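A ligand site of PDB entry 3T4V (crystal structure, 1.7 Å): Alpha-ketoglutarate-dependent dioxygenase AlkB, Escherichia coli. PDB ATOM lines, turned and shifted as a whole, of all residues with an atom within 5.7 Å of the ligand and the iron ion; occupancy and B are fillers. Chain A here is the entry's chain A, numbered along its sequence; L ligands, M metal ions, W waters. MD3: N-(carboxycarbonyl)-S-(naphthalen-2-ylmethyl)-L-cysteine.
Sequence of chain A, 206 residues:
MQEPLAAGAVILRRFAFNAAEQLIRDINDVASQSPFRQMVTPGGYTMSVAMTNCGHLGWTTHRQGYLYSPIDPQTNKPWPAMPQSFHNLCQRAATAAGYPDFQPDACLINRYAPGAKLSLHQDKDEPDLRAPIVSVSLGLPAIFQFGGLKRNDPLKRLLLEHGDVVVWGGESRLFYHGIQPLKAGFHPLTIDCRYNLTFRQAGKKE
The side-chain hydroxyl of Thr 198 sits at hydrogen-bond distance from an oxygen (O05) of the ligand, at 3.3 Å.
The side-chain amide oxygen of Asn 110 lies close to an oxygen (OXT) of the ligand, at 2.9 Å.
The side-chain amide oxygen (OD1) of Asn 196 lies close to an oxygen (OXT) of the ligand, 3.5 Å away.
The guanidinium group (NH2) of Arg 200 is in salt-bridge range of an oxygen (O05) of the ligand (2.9 Å).
OH of Tyr 112 is in hydrogen-bond range of OXT of the ligand.
An oxygen (O) of the ligand is in salt-bridge range of the guanidinium group (NH1) of Arg 194 (2.7 Å).
NH2 of Arg 194 lies close to ND2 of Asn 196 (3.3 Å).
O of Leu 108 lies within hydrogen-bond range of N of Thr 198, 2.9 Å away.
O of Arg 194 sits at hydrogen-bond distance from N of Tyr 112.
The backbone NH of Trp 168 lies within hydrogen-bond range of the backbone carbonyl oxygen of Ile 133.
The backbone NH (N) of Ile 179 lies within hydrogen-bond range of the backbone carbonyl oxygen (O) of Leu 118 (2.9 Å).
NH1 of Arg 200 lies within salt-bridge range of OD2 of Asp 123, 3.0 Å away.
A ring nitrogen (ND1) of His 177 is in hydrogen-bond range of the backbone carbonyl oxygen (O) of Phe 175, 2.9 Å away.
The side-chain hydroxyl (OG) of Ser 137 is in hydrogen-bond range of the guanidinium group (NH2) of Arg 194, at 2.9 Å.
CD2 of Leu 108 touches O05 of the ligand, 3.9 Å away.
CD2 of Leu 118 touches O03 of the ligand, at 3.6 Å.
Ile 133 touches the ligand (CD1 to C13, 3.6 Å).
Ser 135 touches the ligand (OG to C06, 3.7 Å).
Phe 144 touches the ligand.
CE2 of Trp 168 touches C11 of the ligand, 3.2 Å away.
Ser 172 touches the ligand (O to C15, 3.5 Å).
O of Arg 173 touches C14 of the ligand, at 3.4 Å.
Ile 179 touches the ligand (CG1 to O, 3.4 Å).
Within 4 Å of the ligand: Leu 108, Asn 110, Tyr 112, Leu 118, His 121, Asp 123, Ile 133, Ser 135, Phe 144, Trp 168, Ser 172, Arg 173, His 177, Ile 179, Arg 194, Asn 196, Thr 198 and Arg 200.
Along chain A the residues within 4 Å of the ligand span positions 108 to 200.
The nearest printed residue that does not touch the ligand is Leu 160 (4.2 Å).
Within 4 Å of the iron ion: His 121, Asp 123 and His 177.
NE2 of His 177 binds the iron ion, 2.1 Å away.
O04 of the ligand binds the iron ion (2.1 Å).
The iron ion is bound by the side-chain carboxylate (OD1) of Asp 123 (2.1 Å).
The iron ion is bound by NE2 of His 121.
The iron ion is bound by an oxygen (O03) of the ligand (2.2 Å).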
ATOM      1  N   LEU A 108      32.993 -16.761  34.469  1.00  0.00           N
ATOM      2  CA  LEU A 108      33.570 -18.111  34.531  1.00  0.00           C
ATOM      3  C   LEU A 108      34.739 -18.149  33.564  1.00  0.00           C
ATOM      4  O   LEU A 108      34.614 -17.684  32.440  1.00  0.00           O
ATOM      5  CB  LEU A 108      32.530 -19.163  34.112  1.00  0.00           C
ATOM      6  CG  LEU A 108      32.986 -20.621  33.992  1.00  0.00           C
ATOM      7  CD1 LEU A 108      33.387 -21.127  35.347  1.00  0.00           C
ATOM      8  CD2 LEU A 108      31.834 -21.502  33.450  1.00  0.00           C
ATOM      9  N   ASN A 110      37.232 -20.548  31.669  1.00  0.00           N
ATOM     10  CA  ASN A 110      37.460 -21.932  31.204  1.00  0.00           C
ATOM     11  C   ASN A 110      38.845 -22.042  30.575  1.00  0.00           C
ATOM     12  O   ASN A 110      39.183 -21.265  29.680  1.00  0.00           O
ATOM     13  CB  ASN A 110      36.406 -22.321  30.147  1.00  0.00           C
ATOM     14  CG  ASN A 110      35.020 -22.581  30.740  1.00  0.00           C
ATOM     15  OD1 ASN A 110      33.999 -22.685  30.000  1.00  0.00           O
ATOM     16  ND2 ASN A 110      34.953 -22.699  32.034  1.00  0.00           N
ATOM     17  N   TYR A 112      41.292 -24.646  28.404  1.00  0.00           N
ATOM     18  CA  TYR A 112      41.411 -25.846  27.552  1.00  0.00           C
ATOM     19  C   TYR A 112      42.851 -26.191  27.236  1.00  0.00           C
ATOM     20  O   TYR A 112      43.522 -25.465  26.479  1.00  0.00           O
ATOM     21  CB  TYR A 112      40.718 -25.622  26.180  1.00  0.00           C
ATOM     22  CG  TYR A 112      39.230 -25.376  26.364  1.00  0.00           C
ATOM     23  CD1 TYR A 112      38.748 -24.160  26.807  1.00  0.00           C
ATOM     24  CD2 TYR A 112      38.299 -26.380  26.064  1.00  0.00           C
ATOM     25  CE1 TYR A 112      37.378 -23.940  26.992  1.00  0.00           C
ATOM     26  CE2 TYR A 112      36.933 -26.179  26.263  1.00  0.00           C
ATOM     27  CZ  TYR A 112      36.490 -24.950  26.717  1.00  0.00           C
ATOM     28  OH  TYR A 112      35.156 -24.761  26.905  1.00  0.00           O
ATOM     29  N   LEU A 118      33.946 -29.361  25.840  1.00  0.00           N
ATOM     30  CA  LEU A 118      32.837 -29.036  26.692  1.00  0.00           C
ATOM     31  C   LEU A 118      31.593 -29.596  26.008  1.00  0.00           C
ATOM     32  O   LEU A 118      31.261 -29.221  24.881  1.00  0.00           O
ATOM     33  CB  LEU A 118      32.750 -27.519  26.863  1.00  0.00           C
ATOM     34  CG  LEU A 118      31.915 -26.998  28.018  1.00  0.00           C
ATOM     35  CD1 LEU A 118      32.495 -27.482  29.368  1.00  0.00           C
ATOM     36  CD2 LEU A 118      31.869 -25.497  27.949  1.00  0.00           C
ATOM     37  N   HIS A 121      25.371 -28.444  26.009  1.00  0.00           N
ATOM     38  CA  HIS A 121      24.571 -28.044  27.167  1.00  0.00           C
ATOM     39  C   HIS A 121      23.902 -26.718  26.859  1.00  0.00           C
ATOM     40  O   HIS A 121      24.245 -26.043  25.878  1.00  0.00           O
ATOM     41  CB  HIS A 121      25.451 -27.865  28.394  1.00  0.00           C
ATOM     42  CG  HIS A 121      26.413 -26.729  28.258  1.00  0.00           C
ATOM     43  ND1 HIS A 121      27.593 -26.856  27.550  1.00  0.00           N
ATOM     44  CD2 HIS A 121      26.346 -25.449  28.669  1.00  0.00           C
ATOM     45  CE1 HIS A 121      28.219 -25.688  27.550  1.00  0.00           C
ATOM     46  NE2 HIS A 121      27.483 -24.826  28.216  1.00  0.00           N
ATOM     47  N   GLN A 122      22.930 -26.365  27.703  1.00  0.00           N
ATOM     48  CA  GLN A 122      22.352 -25.026  27.771  1.00  0.00           C
ATOM     49  C   GLN A 122      22.863 -24.364  29.025  1.00  0.00           C
ATOM     50  O   GLN A 122      23.145 -25.038  30.033  1.00  0.00           O
ATOM     51  CB  GLN A 122      20.822 -25.111  27.853  1.00  0.00           C
ATOM     52  CG  GLN A 122      20.168 -25.577  26.572  1.00  0.00           C
ATOM     53  CD  GLN A 122      18.673 -25.665  26.714  1.00  0.00           C
ATOM     54  OE1 GLN A 122      18.173 -26.413  27.546  1.00  0.00           O
ATOM     55  NE2 GLN A 122      17.942 -24.881  25.920  1.00  0.00           N
ATOM     56  N   ASP A 123      22.955 -23.028  29.011  1.00  0.00           N
ATOM     57  CA  ASP A 123      23.158 -22.363  30.269  1.00  0.00           C
ATOM     58  C   ASP A 123      21.803 -21.843  30.692  1.00  0.00           C
ATOM     59  O   ASP A 123      21.271 -20.856  30.161  1.00  0.00           O
ATOM     60  CB  ASP A 123      24.097 -21.194  30.018  1.00  0.00           C
ATOM     61  CG  ASP A 123      25.528 -21.652  29.873  1.00  0.00           C
ATOM     62  OD1 ASP A 123      25.869 -22.089  28.768  1.00  0.00           O
ATOM     63  OD2 ASP A 123      26.283 -21.577  30.865  1.00  0.00           O
ATOM     64  N   ILE A 133      24.735 -13.631  27.707  1.00  0.00           N
ATOM     65  CA  ILE A 133      26.049 -13.994  28.191  1.00  0.00           C
ATOM     66  C   ILE A 133      27.058 -13.494  27.191  1.00  0.00           C
ATOM     67  O   ILE A 133      26.827 -13.600  25.967  1.00  0.00           O
ATOM     68  CB  ILE A 133      26.153 -15.528  28.449  1.00  0.00           C
ATOM     69  CG1 ILE A 133      25.320 -15.919  29.691  1.00  0.00           C
ATOM     70  CG2 ILE A 133      27.625 -16.005  28.616  1.00  0.00           C
ATOM     71  CD1 ILE A 133      25.219 -17.439  29.988  1.00  0.00           C
ATOM     72  N   SER A 135      30.901 -14.027  25.744  1.00  0.00           N
ATOM     73  CA  SER A 135      32.116 -14.846  25.758  1.00  0.00           C
ATOM     74  C   SER A 135      33.285 -14.131  25.099  1.00  0.00           C
ATOM     75  O   SER A 135      33.109 -13.359  24.134  1.00  0.00           O
ATOM     76  CB  SER A 135      31.903 -16.195  25.018  1.00  0.00           C
ATOM     77  OG  SER A 135      31.587 -15.964  23.648  1.00  0.00           O
ATOM     78  N   SER A 137      37.175 -15.240  23.720  1.00  0.00           N
ATOM     79  CA  SER A 137      38.060 -16.384  23.442  1.00  0.00           C
ATOM     80  C   SER A 137      39.479 -15.864  23.279  1.00  0.00           C
ATOM     81  O   SER A 137      39.708 -14.821  22.669  1.00  0.00           O
ATOM     82  CB  SER A 137      37.617 -17.132  22.180  1.00  0.00           C
ATOM     83  OG  SER A 137      36.318 -17.688  22.363  1.00  0.00           O
ATOM     84  N   PHE A 144      33.389 -24.299  17.936  1.00  0.00           N
ATOM     85  CA  PHE A 144      32.166 -24.141  18.722  1.00  0.00           C
ATOM     86  C   PHE A 144      30.980 -24.748  17.994  1.00  0.00           C
ATOM     87  O   PHE A 144      30.748 -24.480  16.799  1.00  0.00           O
ATOM     88  CB  PHE A 144      31.973 -22.633  18.961  1.00  0.00           C
ATOM     89  CG  PHE A 144      30.657 -22.254  19.601  1.00  0.00           C
ATOM     90  CD1 PHE A 144      30.454 -22.437  20.974  1.00  0.00           C
ATOM     91  CD2 PHE A 144      29.653 -21.680  18.836  1.00  0.00           C
ATOM     92  CE1 PHE A 144      29.251 -22.072  21.567  1.00  0.00           C
ATOM     93  CE2 PHE A 144      28.449 -21.311  19.420  1.00  0.00           C
ATOM     94  CZ  PHE A 144      28.238 -21.513  20.784  1.00  0.00           C
ATOM     95  N   LEU A 160      36.081 -20.347  16.904  1.00  0.00           N
ATOM     96  CA  LEU A 160      36.265 -19.179  17.762  1.00  0.00           C
ATOM     97  C   LEU A 160      37.778 -19.000  17.887  1.00  0.00           C
ATOM     98  O   LEU A 160      38.494 -19.927  18.274  1.00  0.00           O
ATOM     99  CB  LEU A 160      35.602 -19.365  19.124  1.00  0.00           C
ATOM    100  CG  LEU A 160      34.062 -19.399  19.041  1.00  0.00           C
ATOM    101  CD1 LEU A 160      33.489 -19.782  20.394  1.00  0.00           C
ATOM    102  CD2 LEU A 160      33.498 -18.018  18.598  1.00  0.00           C
ATOM    103  N   TRP A 168      25.766 -13.349  23.403  1.00  0.00           N
ATOM    104  CA  TRP A 168      24.732 -14.305  23.064  1.00  0.00           C
ATOM    105  C   TRP A 168      23.425 -13.820  23.699  1.00  0.00           C
ATOM    106  O   TRP A 168      23.156 -14.031  24.888  1.00  0.00           O
ATOM    107  CB  TRP A 168      25.178 -15.657  23.698  1.00  0.00           C
ATOM    108  CG  TRP A 168      26.532 -16.135  23.217  1.00  0.00           C
ATOM    109  CD1 TRP A 168      27.757 -15.961  23.824  1.00  0.00           C
ATOM    110  CD2 TRP A 168      26.795 -16.823  21.999  1.00  0.00           C
ATOM    111  NE1 TRP A 168      28.762 -16.513  23.045  1.00  0.00           N
ATOM    112  CE2 TRP A 168      28.191 -17.043  21.911  1.00  0.00           C
ATOM    113  CE3 TRP A 168      25.966 -17.268  20.948  1.00  0.00           C
ATOM    114  CZ2 TRP A 168      28.773 -17.706  20.837  1.00  0.00           C
ATOM    115  CZ3 TRP A 168      26.548 -17.927  19.887  1.00  0.00           C
ATOM    116  CH2 TRP A 168      27.935 -18.140  19.826  1.00  0.00           C
ATOM    117  N   SER A 172      19.542 -17.048  20.765  1.00  0.00           N
ATOM    118  CA  SER A 172      20.775 -17.786  20.850  1.00  0.00           C
ATOM    119  C   SER A 172      21.158 -18.022  22.297  1.00  0.00           C
ATOM    120  O   SER A 172      21.922 -18.961  22.591  1.00  0.00           O
ATOM    121  CB  SER A 172      21.915 -17.044  20.129  1.00  0.00           C
ATOM    122  OG  SER A 172      22.415 -15.991  20.937  1.00  0.00           O
ATOM    123  N   ARG A 173      20.660 -17.167  23.183  1.00  0.00           N
ATOM    124  CA  ARG A 173      20.981 -17.301  24.611  1.00  0.00           C
ATOM    125  C   ARG A 173      20.571 -18.689  25.145  1.00  0.00           C
ATOM    126  O   ARG A 173      21.180 -19.225  26.104  1.00  0.00           O
ATOM    127  CB  ARG A 173      20.267 -16.167  25.354  1.00  0.00           C
ATOM    128  CG  ARG A 173      20.331 -16.217  26.864  1.00  0.00           C
ATOM    129  CD  ARG A 173      21.743 -15.982  27.394  1.00  0.00           C
ATOM    130  NE  ARG A 173      21.670 -16.026  28.849  1.00  0.00           N
ATOM    131  CZ  ARG A 173      21.699 -17.165  29.529  1.00  0.00           C
ATOM    132  NH1 ARG A 173      21.837 -18.309  28.860  1.00  0.00           N
ATOM    133  NH2 ARG A 173      21.629 -17.161  30.850  1.00  0.00           N
ATOM    134  N   LEU A 174      19.541 -19.280  24.525  1.00  0.00           N
ATOM    135  CA  LEU A 174      18.994 -20.584  24.920  1.00  0.00           C
ATOM    136  C   LEU A 174      19.494 -21.782  24.122  1.00  0.00           C
ATOM    137  O   LEU A 174      18.988 -22.883  24.317  1.00  0.00           O
ATOM    138  CB  LEU A 174      17.471 -20.600  24.831  1.00  0.00           C
ATOM    139  CG  LEU A 174      16.729 -19.638  25.740  1.00  0.00           C
ATOM    140  CD1 LEU A 174      15.275 -20.050  25.839  1.00  0.00           C
ATOM    141  CD2 LEU A 174      17.381 -19.606  27.110  1.00  0.00           C
ATOM    142  N   PHE A 175      20.388 -21.565  23.167  1.00  0.00           N
ATOM    143  CA  PHE A 175      20.780 -22.665  22.277  1.00  0.00           C
ATOM    144  C   PHE A 175      21.608 -23.679  23.065  1.00  0.00           C
ATOM    145  O   PHE A 175      22.401 -23.312  23.948  1.00  0.00           O
ATOM    146  CB  PHE A 175      21.679 -22.165  21.135  1.00  0.00           C
ATOM    147  CG  PHE A 175      20.940 -21.484  20.010  1.00  0.00           C
ATOM    148  CD1 PHE A 175      21.661 -20.880  18.981  1.00  0.00           C
ATOM    149  CD2 PHE A 175      19.569 -21.426  19.980  1.00  0.00           C
ATOM    150  CE1 PHE A 175      21.006 -20.242  17.922  1.00  0.00           C
ATOM    151  CE2 PHE A 175      18.904 -20.786  18.935  1.00  0.00           C
ATOM    152  CZ  PHE A 175      19.648 -20.196  17.896  1.00  0.00           C
ATOM    153  N   HIS A 177      24.888 -25.791  23.119  1.00  0.00           N
ATOM    154  CA  HIS A 177      26.171 -25.433  22.502  1.00  0.00           C
ATOM    155  C   HIS A 177      27.267 -26.171  23.239  1.00  0.00           C
ATOM    156  O   HIS A 177      27.045 -26.695  24.343  1.00  0.00           O
ATOM    157  CB  HIS A 177      26.396 -23.921  22.565  1.00  0.00           C
ATOM    158  CG  HIS A 177      26.389 -23.391  23.969  1.00  0.00           C
ATOM    159  ND1 HIS A 177      25.220 -23.121  24.645  1.00  0.00           N
ATOM    160  CD2 HIS A 177      27.399 -23.190  24.849  1.00  0.00           C
ATOM    161  CE1 HIS A 177      25.518 -22.733  25.875  1.00  0.00           C
ATOM    162  NE2 HIS A 177      26.830 -22.768  26.015  1.00  0.00           N
ATOM    163  N   GLY A 178      28.466 -26.204  22.643  1.00  0.00           N
ATOM    164  CA  GLY A 178      29.607 -26.835  23.280  1.00  0.00           C
ATOM    165  C   GLY A 178      30.888 -26.567  22.505  1.00  0.00           C
ATOM    166  O   GLY A 178      30.895 -25.849  21.508  1.00  0.00           O
ATOM    167  N   ILE A 179      31.983 -27.173  22.947  1.00  0.00           N
ATOM    168  CA  ILE A 179      33.304 -26.958  22.331  1.00  0.00           C
ATOM    169  C   ILE A 179      33.872 -28.356  22.044  1.00  0.00           C
ATOM    170  O   ILE A 179      33.859 -29.228  22.920  1.00  0.00           O
ATOM    171  CB  ILE A 179      34.241 -26.212  23.279  1.00  0.00           C
ATOM    172  CG1 ILE A 179      33.743 -24.777  23.473  1.00  0.00           C
ATOM    173  CG2 ILE A 179      35.702 -26.208  22.762  1.00  0.00           C
ATOM    174  CD1 ILE A 179      33.989 -23.849  22.217  1.00  0.00           C
ATOM    175  N   ARG A 194      43.796 -22.732  25.361  1.00  0.00           N
ATOM    176  CA  ARG A 194      42.775 -21.726  25.095  1.00  0.00           C
ATOM    177  C   ARG A 194      42.107 -21.289  26.397  1.00  0.00           C
ATOM    178  O   ARG A 194      41.891 -22.105  27.298  1.00  0.00           O
ATOM    179  CB  ARG A 194      41.720 -22.336  24.154  1.00  0.00           C
ATOM    180  CG  ARG A 194      40.471 -21.449  23.954  1.00  0.00           C
ATOM    181  CD  ARG A 194      39.540 -22.060  22.858  1.00  0.00           C
ATOM    182  NE  ARG A 194      38.372 -21.216  22.658  1.00  0.00           N
ATOM    183  CZ  ARG A 194      37.190 -21.371  23.248  1.00  0.00           C
ATOM    184  NH1 ARG A 194      36.977 -22.374  24.113  1.00  0.00           N
ATOM    185  NH2 ARG A 194      36.216 -20.498  22.988  1.00  0.00           N
ATOM    186  N   ASN A 196      38.601 -19.170  27.802  1.00  0.00           N
ATOM    187  CA  ASN A 196      37.343 -18.546  27.427  1.00  0.00           C
ATOM    188  C   ASN A 196      36.713 -17.904  28.656  1.00  0.00           C
ATOM    189  O   ASN A 196      36.562 -18.550  29.689  1.00  0.00           O
ATOM    190  CB  ASN A 196      36.363 -19.543  26.812  1.00  0.00           C
ATOM    191  CG  ASN A 196      35.112 -18.876  26.334  1.00  0.00           C
ATOM    192  OD1 ASN A 196      34.106 -18.861  27.027  1.00  0.00           O
ATOM    193  ND2 ASN A 196      35.176 -18.295  25.159  1.00  0.00           N
ATOM    194  N   THR A 198      33.356 -16.228  30.257  1.00  0.00           N
ATOM    195  CA  THR A 198      31.921 -15.948  30.044  1.00  0.00           C
ATOM    196  C   THR A 198      31.352 -15.123  31.185  1.00  0.00           C
ATOM    197  O   THR A 198      31.355 -15.536  32.344  1.00  0.00           O
ATOM    198  CB  THR A 198      31.048 -17.212  29.865  1.00  0.00           C
ATOM    199  OG1 THR A 198      31.377 -18.169  30.883  1.00  0.00           O
ATOM    200  CG2 THR A 198      31.240 -17.843  28.495  1.00  0.00           C
ATOM    201  N   ARG A 200      28.309 -13.353  33.078  1.00  0.00           N
ATOM    202  CA  ARG A 200      26.889 -13.679  33.372  1.00  0.00           C
ATOM    203  C   ARG A 200      26.310 -12.732  34.406  1.00  0.00           C
ATOM    204  O   ARG A 200      27.033 -12.314  35.303  1.00  0.00           O
ATOM    205  CB  ARG A 200      26.836 -15.097  33.971  1.00  0.00           C
ATOM    206  CG  ARG A 200      27.407 -16.184  33.026  1.00  0.00           C
ATOM    207  CD  ARG A 200      28.471 -17.036  33.689  1.00  0.00           C
ATOM    208  NE  ARG A 200      29.070 -17.966  32.716  1.00  0.00           N
ATOM    209  CZ  ARG A 200      28.426 -19.026  32.221  1.00  0.00           C
ATOM    210  NH1 ARG A 200      27.170 -19.279  32.605  1.00  0.00           N
ATOM    211  NH2 ARG A 200      29.021 -19.812  31.320  1.00  0.00           N
HETATM  212  C16 MD3 L   1      25.642 -19.470  24.131  1.00  0.00           C
HETATM  213  N   MD3 L   1      31.737 -21.902  27.188  1.00  0.00           N
HETATM  214  O05 MD3 L   1      30.923 -21.218  29.672  1.00  0.00           O
HETATM  215  SG  MD3 L   1      32.112 -20.023  24.310  1.00  0.00           S
HETATM  216  C01 MD3 L   1      30.018 -21.742  28.965  1.00  0.00           C
HETATM  217  OXT MD3 L   1      34.331 -22.329  27.161  1.00  0.00           O
HETATM  218  C02 MD3 L   1      30.426 -22.226  27.623  1.00  0.00           C
HETATM  219  O   MD3 L   1      34.468 -21.861  25.049  1.00  0.00           O
HETATM  220  CA  MD3 L   1      32.294 -22.335  25.950  1.00  0.00           C
HETATM  221  O03 MD3 L   1      29.671 -22.877  26.965  1.00  0.00           O
HETATM  222  C   MD3 L   1      33.776 -22.158  26.046  1.00  0.00           C
HETATM  223  O04 MD3 L   1      28.826 -21.897  29.377  1.00  0.00           O
HETATM  224  CB  MD3 L   1      31.745 -21.719  24.706  1.00  0.00           C
HETATM  225  C06 MD3 L   1      30.557 -19.468  23.665  1.00  0.00           C
HETATM  226  C07 MD3 L   1      29.332 -19.431  24.527  1.00  0.00           C
HETATM  227  C08 MD3 L   1      29.434 -19.302  25.906  1.00  0.00           C
HETATM  228  C09 MD3 L   1      28.278 -19.227  26.674  1.00  0.00           C
HETATM  229  C10 MD3 L   1      27.012 -19.286  26.096  1.00  0.00           C
HETATM  230  C11 MD3 L   1      28.072 -19.479  23.930  1.00  0.00           C
HETATM  231  C12 MD3 L   1      26.906 -19.402  24.713  1.00  0.00           C
HETATM  232  C13 MD3 L   1      25.851 -19.235  26.888  1.00  0.00           C
HETATM  233  C14 MD3 L   1      24.591 -19.275  26.296  1.00  0.00           C
HETATM  234  C15 MD3 L   1      24.490 -19.416  24.899  1.00  0.00           C
HETATM  235 FE    FE M   1      27.673 -22.737  27.885  1.00  0.00          FE
HETATM  236  O   HOH W   1      33.614 -19.502  30.009  1.00  0.00           O
